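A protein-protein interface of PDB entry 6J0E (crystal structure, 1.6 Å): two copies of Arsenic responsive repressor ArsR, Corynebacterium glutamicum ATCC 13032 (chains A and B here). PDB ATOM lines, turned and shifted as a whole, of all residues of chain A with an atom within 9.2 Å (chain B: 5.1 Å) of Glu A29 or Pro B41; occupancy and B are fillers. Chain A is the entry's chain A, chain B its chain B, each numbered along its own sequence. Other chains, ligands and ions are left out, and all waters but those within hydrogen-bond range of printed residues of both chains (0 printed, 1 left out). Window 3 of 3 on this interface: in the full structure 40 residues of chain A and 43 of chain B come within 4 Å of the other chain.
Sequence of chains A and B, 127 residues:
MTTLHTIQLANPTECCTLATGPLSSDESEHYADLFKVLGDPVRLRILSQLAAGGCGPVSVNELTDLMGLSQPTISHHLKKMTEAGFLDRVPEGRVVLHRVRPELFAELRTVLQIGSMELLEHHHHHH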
ATOM      1  N   LEU A  23      21.713  31.394  -5.051  1.00  0.00           N
ATOM      2  CA  LEU A  23      21.681  30.430  -3.978  1.00  0.00           C
ATOM      3  C   LEU A  23      22.195  29.118  -4.527  1.00  0.00           C
ATOM      4  O   LEU A  23      22.047  28.828  -5.739  1.00  0.00           O
ATOM      5  CB  LEU A  23      20.214  30.240  -3.437  1.00  0.00           C
ATOM      6  CG  LEU A  23      19.470  31.346  -2.668  1.00  0.00           C
ATOM      7  CD1 LEU A  23      17.953  31.074  -2.666  1.00  0.00           C
ATOM      8  CD2 LEU A  23      19.953  31.544  -1.243  1.00  0.00           C
ATOM      9  N   SER A  24      22.830  28.329  -3.653  1.00  0.00           N
ATOM     10  CA  SER A  24      23.299  27.066  -4.038  1.00  0.00           C
ATOM     11  C   SER A  24      22.204  26.027  -4.033  1.00  0.00           C
ATOM     12  O   SER A  24      21.032  26.311  -3.646  1.00  0.00           O
ATOM     13  CB  SER A  24      24.428  26.629  -3.092  1.00  0.00           C
ATOM     14  OG  SER A  24      23.928  26.402  -1.774  1.00  0.00           O
ATOM     15  N   SER A  25      22.538  24.864  -4.559  1.00  0.00           N
ATOM     16  CA  SER A  25      21.581  23.739  -4.551  1.00  0.00           C
ATOM     17  C   SER A  25      20.990  23.476  -3.139  1.00  0.00           C
ATOM     18  O   SER A  25      19.763  23.368  -3.016  1.00  0.00           O
ATOM     19  CB  SER A  25      22.215  22.483  -5.115  1.00  0.00           C
ATOM     20  OG  SER A  25      21.218  21.491  -5.257  1.00  0.00           O
ATOM     21  N   ASP A  26      21.855  23.367  -2.110  1.00  0.00           N
ATOM     22  CA  ASP A  26      21.439  23.045  -0.708  1.00  0.00           C
ATOM     23  C   ASP A  26      20.718  24.171   0.007  1.00  0.00           C
ATOM     24  O   ASP A  26      19.638  23.940   0.633  1.00  0.00           O
ATOM     25  CB  ASP A  26      22.691  22.760   0.172  1.00  0.00           C
ATOM     26  CG  ASP A  26      23.417  21.539  -0.245  1.00  0.00           C
ATOM     27  OD1 ASP A  26      22.771  20.625  -0.805  1.00  0.00           O
ATOM     28  OD2 ASP A  26      24.637  21.527  -0.061  1.00  0.00           O
ATOM     29  N   GLU A  27      21.278  25.383  -0.059  1.00  0.00           N
ATOM     30  CA  GLU A  27      20.593  26.597   0.464  1.00  0.00           C
ATOM     31  C   GLU A  27      19.165  26.748  -0.181  1.00  0.00           C
ATOM     32  O   GLU A  27      18.196  26.939   0.556  1.00  0.00           O
ATOM     33  CB  GLU A  27      21.315  27.911   0.249  1.00  0.00           C
ATOM     34  CG  GLU A  27      22.685  28.084   0.778  1.00  0.00           C
ATOM     35  CD  GLU A  27      23.388  29.212   0.066  1.00  0.00           C
ATOM     36  OE1 GLU A  27      23.149  29.525  -1.140  1.00  0.00           O
ATOM     37  OE2 GLU A  27      24.284  29.780   0.691  1.00  0.00           O
ATOM     38  N   SER A  28      19.074  26.546  -1.495  1.00  0.00           N
ATOM     39  CA  SER A  28      17.723  26.502  -2.205  1.00  0.00           C
ATOM     40  C   SER A  28      16.783  25.348  -1.662  1.00  0.00           C
ATOM     41  O   SER A  28      15.500  25.559  -1.474  1.00  0.00           O
ATOM     42  CB  SER A  28      17.882  26.429  -3.775  1.00  0.00           C
ATOM     43  OG  SER A  28      18.060  25.065  -4.323  1.00  0.00           O
ATOM     44  N   GLU A  29      17.358  24.143  -1.424  1.00  0.00           N
ATOM     45  CA  GLU A  29      16.594  23.016  -0.912  1.00  0.00           C
ATOM     46  C   GLU A  29      16.094  23.381   0.500  1.00  0.00           C
ATOM     47  O   GLU A  29      14.907  23.142   0.837  1.00  0.00           O
ATOM     48  CB  GLU A  29      17.444  21.691  -0.888  1.00  0.00           C
ATOM     49  CG  GLU A  29      17.744  21.046  -2.259  1.00  0.00           C
ATOM     50  CD  GLU A  29      16.569  20.383  -2.917  1.00  0.00           C
ATOM     51  OE1 GLU A  29      15.625  19.975  -2.184  1.00  0.00           O
ATOM     52  OE2 GLU A  29      16.603  20.299  -4.178  1.00  0.00           O
ATOM     53  N   HIS A  30      16.986  23.932   1.295  1.00  0.00           N
ATOM     54  CA  HIS A  30      16.655  24.333   2.699  1.00  0.00           C
ATOM     55  C   HIS A  30      15.473  25.367   2.765  1.00  0.00           C
ATOM     56  O   HIS A  30      14.471  25.183   3.519  1.00  0.00           O
ATOM     57  CB  HIS A  30      17.887  24.993   3.360  1.00  0.00           C
ATOM     58  CG  HIS A  30      17.650  25.460   4.779  1.00  0.00           C
ATOM     59  ND1 HIS A  30      16.933  24.714   5.703  1.00  0.00           N
ATOM     60  CD2 HIS A  30      17.929  26.636   5.405  1.00  0.00           C
ATOM     61  CE1 HIS A  30      16.850  25.375   6.836  1.00  0.00           C
ATOM     62  NE2 HIS A  30      17.447  26.536   6.691  1.00  0.00           N
ATOM     63  N   TYR A  31      15.639  26.515   2.072  1.00  0.00           N
ATOM     64  CA  TYR A  31      14.584  27.542   2.128  1.00  0.00           C
ATOM     65  C   TYR A  31      13.308  27.100   1.489  1.00  0.00           C
ATOM     66  O   TYR A  31      12.269  27.417   2.040  1.00  0.00           O
ATOM     67  CB  TYR A  31      15.079  28.955   1.627  1.00  0.00           C
ATOM     68  CG  TYR A  31      16.179  29.428   2.560  1.00  0.00           C
ATOM     69  CD1 TYR A  31      15.928  29.642   3.970  1.00  0.00           C
ATOM     70  CD2 TYR A  31      17.488  29.561   2.126  1.00  0.00           C
ATOM     71  CE1 TYR A  31      16.861  30.041   4.865  1.00  0.00           C
ATOM     72  CE2 TYR A  31      18.466  29.944   3.048  1.00  0.00           C
ATOM     73  CZ  TYR A  31      18.186  30.190   4.418  1.00  0.00           C
ATOM     74  OH  TYR A  31      19.156  30.553   5.369  1.00  0.00           O
ATOM     75  N   ALA A  32      13.337  26.344   0.371  1.00  0.00           N
ATOM     76  CA  ALA A  32      12.196  25.692  -0.132  1.00  0.00           C
ATOM     77  C   ALA A  32      11.440  24.910   0.969  1.00  0.00           C
ATOM     78  O   ALA A  32      10.125  25.018   1.096  1.00  0.00           O
ATOM     79  CB  ALA A  32      12.476  24.770  -1.319  1.00  0.00           C
ATOM     80  N   ASP A  33      12.245  24.143   1.743  1.00  0.00           N
ATOM     81  CA  ASP A  33      11.600  23.349   2.786  1.00  0.00           C
ATOM     82  C   ASP A  33      10.887  24.175   3.790  1.00  0.00           C
ATOM     83  O   ASP A  33       9.774  23.878   4.183  1.00  0.00           O
ATOM     84  CB  ASP A  33      12.642  22.488   3.647  1.00  0.00           C
ATOM     85  CG  ASP A  33      13.391  21.484   2.899  1.00  0.00           C
ATOM     86  OD1 ASP A  33      12.934  21.065   1.840  1.00  0.00           O
ATOM     87  OD2 ASP A  33      14.483  21.031   3.415  1.00  0.00           O
ATOM     88  N   LEU A  34      11.496  25.289   4.180  1.00  0.00           N
ATOM     89  CA  LEU A  34      10.801  26.196   5.056  1.00  0.00           C
ATOM     90  C   LEU A  34       9.530  26.905   4.528  1.00  0.00           C
ATOM     91  O   LEU A  34       8.512  26.993   5.153  1.00  0.00           O
ATOM     92  CB  LEU A  34      11.817  27.241   5.569  1.00  0.00           C
ATOM     93  CG  LEU A  34      13.018  26.794   6.477  1.00  0.00           C
ATOM     94  CD1 LEU A  34      13.888  27.919   6.935  1.00  0.00           C
ATOM     95  CD2 LEU A  34      12.439  26.047   7.657  1.00  0.00           C
ATOM     96  N   PHE A  35       9.641  27.333   3.240  1.00  0.00           N
ATOM     97  CA  PHE A  35       8.459  27.896   2.593  1.00  0.00           C
ATOM     98  C   PHE A  35       7.319  26.881   2.457  1.00  0.00           C
ATOM     99  O   PHE A  35       6.201  27.263   2.560  1.00  0.00           O
ATOM    100  CB  PHE A  35       8.819  28.536   1.211  1.00  0.00           C
ATOM    101  CG  PHE A  35       9.543  29.865   1.325  1.00  0.00           C
ATOM    102  CD1 PHE A  35       9.032  30.861   2.073  1.00  0.00           C
ATOM    103  CD2 PHE A  35      10.810  30.078   0.637  1.00  0.00           C
ATOM    104  CE1 PHE A  35       9.531  32.111   2.075  1.00  0.00           C
ATOM    105  CE2 PHE A  35      11.385  31.327   0.747  1.00  0.00           C
ATOM    106  CZ  PHE A  35      10.789  32.318   1.466  1.00  0.00           C
ATOM    107  N   LYS A  36       7.651  25.594   2.339  1.00  0.00           N
ATOM    108  CA  LYS A  36       6.672  24.526   2.292  1.00  0.00           C
ATOM    109  C   LYS A  36       5.915  24.456   3.550  1.00  0.00           C
ATOM    110  O   LYS A  36       4.716  24.244   3.531  1.00  0.00           O
ATOM    111  CB  LYS A  36       7.303  23.138   1.952  1.00  0.00           C
ATOM    112  CG  LYS A  36       7.203  22.739   0.527  1.00  0.00           C
ATOM    113  CD  LYS A  36       7.761  21.325   0.331  1.00  0.00           C
ATOM    114  CE  LYS A  36       6.645  20.263   0.489  1.00  0.00           C
ATOM    115  NZ  LYS A  36       7.282  18.878   0.566  1.00  0.00           N
ATOM    116  N   GLY B  39       8.022  27.207  -2.314  1.00  0.00           N
ATOM    117  CA  GLY B  39       8.614  25.994  -1.707  1.00  0.00           C
ATOM    118  C   GLY B  39       9.015  25.042  -2.767  1.00  0.00           C
ATOM    119  O   GLY B  39       8.816  23.896  -2.586  1.00  0.00           O
ATOM    120  N   ASP B  40       9.743  25.470  -3.785  1.00  0.00           N
ATOM    121  CA  ASP B  40      10.363  24.594  -4.761  1.00  0.00           C
ATOM    122  C   ASP B  40      11.821  25.132  -4.928  1.00  0.00           C
ATOM    123  O   ASP B  40      12.011  26.272  -5.244  1.00  0.00           O
ATOM    124  CB  ASP B  40       9.615  24.689  -6.099  1.00  0.00           C
ATOM    125  CG  ASP B  40      10.290  23.876  -7.195  1.00  0.00           C
ATOM    126  OD1 ASP B  40      11.385  24.170  -7.632  1.00  0.00           O
ATOM    127  OD2 ASP B  40       9.721  22.940  -7.650  1.00  0.00           O
ATOM    128  N   PRO B  41      12.812  24.328  -4.781  1.00  0.00           N
ATOM    129  CA  PRO B  41      14.205  24.791  -4.917  1.00  0.00           C
ATOM    130  C   PRO B  41      14.641  25.404  -6.218  1.00  0.00           C
ATOM    131  O   PRO B  41      15.368  26.418  -6.200  1.00  0.00           O
ATOM    132  CB  PRO B  41      15.074  23.494  -4.685  1.00  0.00           C
ATOM    133  CG  PRO B  41      14.103  22.396  -4.504  1.00  0.00           C
ATOM    134  CD  PRO B  41      12.689  22.844  -4.703  1.00  0.00           C
ATOM    135  N   VAL B  42      14.181  24.831  -7.335  1.00  0.00           N
ATOM    136  CA  VAL B  42      14.533  25.344  -8.659  1.00  0.00           C
ATOM    137  C   VAL B  42      13.932  26.792  -8.743  1.00  0.00           C
ATOM    138  O   VAL B  42      14.506  27.713  -9.352  1.00  0.00           O
ATOM    139  CB  VAL B  42      14.098  24.399  -9.801  1.00  0.00           C
ATOM    140  CG1 VAL B  42      14.302  25.031 -11.188  1.00  0.00           C
ATOM    141  CG2 VAL B  42      14.814  23.099  -9.694  1.00  0.00           C
ATOM    142  N   ARG B  43      12.672  26.964  -8.269  1.00  0.00           N
ATOM    143  CA  ARG B  43      12.080  28.302  -8.319  1.00  0.00           C
ATOM    144  C   ARG B  43      12.842  29.316  -7.570  1.00  0.00           C
ATOM    145  O   ARG B  43      13.014  30.445  -7.988  1.00  0.00           O
ATOM    146  CB  ARG B  43      10.598  28.350  -7.813  1.00  0.00           C
ATOM    147  CG  ARG B  43       9.638  27.723  -8.778  1.00  0.00           C
ATOM    148  CD  ARG B  43       8.269  27.497  -8.293  1.00  0.00           C
ATOM    149  NE  ARG B  43       7.673  26.544  -9.181  1.00  0.00           N
ATOM    150  CZ  ARG B  43       6.634  25.789  -8.831  1.00  0.00           C
ATOM    151  NH1 ARG B  43       6.185  25.778  -7.544  1.00  0.00           N
ATOM    152  NH2 ARG B  43       6.112  24.999  -9.769  1.00  0.00           N
ATOM    153  N   LEU B  44      13.333  28.934  -6.440  1.00  0.00           N
ATOM    154  CA  LEU B  44      14.125  29.863  -5.634  1.00  0.00           C
ATOM    155  C   LEU B  44      15.407  30.249  -6.307  1.00  0.00           C
ATOM    156  O   LEU B  44      15.828  31.408  -6.223  1.00  0.00           O
ATOM    157  CB  LEU B  44      14.472  29.226  -4.242  1.00  0.00           C
ATOM    158  CG  LEU B  44      13.258  29.220  -3.358  1.00  0.00           C
ATOM    159  CD1 LEU B  44      13.840  28.873  -1.947  1.00  0.00           C
ATOM    160  CD2 LEU B  44      12.472  30.490  -3.228  1.00  0.00           C
ATOM    161  N   ARG B  45      16.069  29.258  -6.880  1.00  0.00           N
ATOM    162  CA  ARG B  45      17.252  29.542  -7.751  1.00  0.00           C
ATOM    163  C   ARG B  45      17.014  30.414  -8.969  1.00  0.00           C
ATOM    164  O   ARG B  45      17.908  31.227  -9.293  1.00  0.00           O
ATOM    165  CB  ARG B  45      17.939  28.272  -8.168  1.00  0.00           C
ATOM    166  CG  ARG B  45      18.468  27.514  -6.973  1.00  0.00           C
ATOM    167  CD  ARG B  45      19.716  26.627  -7.211  1.00  0.00           C
ATOM    168  NE  ARG B  45      19.532  25.749  -8.351  1.00  0.00           N
ATOM    169  CZ  ARG B  45      18.909  24.578  -8.384  1.00  0.00           C
ATOM    170  NH1 ARG B  45      18.305  24.101  -7.346  1.00  0.00           N
ATOM    171  NH2 ARG B  45      18.840  23.898  -9.537  1.00  0.00           N
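The side-chain hydroxyl (OG) of Ser A28 sits at hydrogen-bond distance from the guanidinium group (NH1) of Arg B45 (3.2 Å).
The side-chain hydroxyl (OG) of Ser A28 sits close to the backbone carbonyl oxygen (O) of Ser A24 (3.3 Å). The backbone NH (N) of Arg B43 is in hydrogen-bond range of the side-chain carboxylate (OD1) of Asp B40, 3.1 Å away. OE1 of Glu A27 sits at hydrogen-bond distance from N of Ser A24, 2.8 Å away. The backbone carbonyl oxygen of Ser A25 lies within hydrogen-bond range of the side-chain hydroxyl of Ser A28 (2.7 Å). OD1 of Asp B40 lies within hydrogen-bond range of N of Val B42 (2.9 Å).
Among the printed residues, merely in contact across the chains: Leu A23 with Arg B45 (3.5 Å), Ser A24 with Arg B45 (3.8 Å), Ser A28 with Pro B41 (3.4 Å), Ser A28 with Leu B44 (3.7 Å), Glu A29 with Pro B41 (3.3 Å), Tyr A31 with Leu B44 (3.8 Å), Ala A32 with Gly B39 (3.3 Å), Ala A32 with Asp B40 (3.7 Å), Ala A32 with Pro B41 (3.5 Å), Ala A32 with Leu B44 (3.5 Å), Phe A35 with Gly B39 (3.9 Å) and Lys A36 with Gly B39 (3.7 Å).
Glu A29 touches one residue of chain B. Of chain A, only Ala A32 comes within 4 Å of Asp B40. Val B42 touches none of the printed residues of chain A. Of the printed residues of chain B, Ser A24 touches Arg B45. Printed residues of chain B within 4 Å of Ala A32: Gly B39 (3.3 Å), Asp B40 (3.7 Å), Pro B41 (3.5 Å) and Leu B44 (3.5 Å). Of the printed residues of chain B, Ser A28 touches Pro B41 (3.4 Å), Leu B44 (3.7 Å) and Arg B45 (3.2 Å). The nearest residue of chain A that does not touch Pro B41 is Ser A25 (5.0 Å).
Of the 7 printed residues of chain B, 5 touch a printed residue of chain A. Printed residues of chain B that touch a printed residue of chain A: Gly B39, Asp B40, Pro B41, Leu B44 and Arg B45. Hydrophobic or aromatic side chains of chain B that line the printed part of chain A: Pro B41 and Leu B44. Of the 14 printed residues of chain A, 8 touch a printed residue of chain B. Printed residues of chain A that touch a printed residue of chain B: Leu A23, Ser A24, Ser A28, Glu A29, Tyr A31, Ala A32, Phe A35 and Lys A36. Hydrophobic or aromatic side chains of chain A that line the printed part of chain B: Tyr A31, Ala A32 and Phe A35. Among the printed residues, no Asp or Glu carboxylate lies within 4 Å of a Lys or Arg side-chain nitrogen of the other chain.
No position is printed for both chains. Of the 13 pairs that touch across the chains among the printed residues, none has its exchanged pair printed and touching as well.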
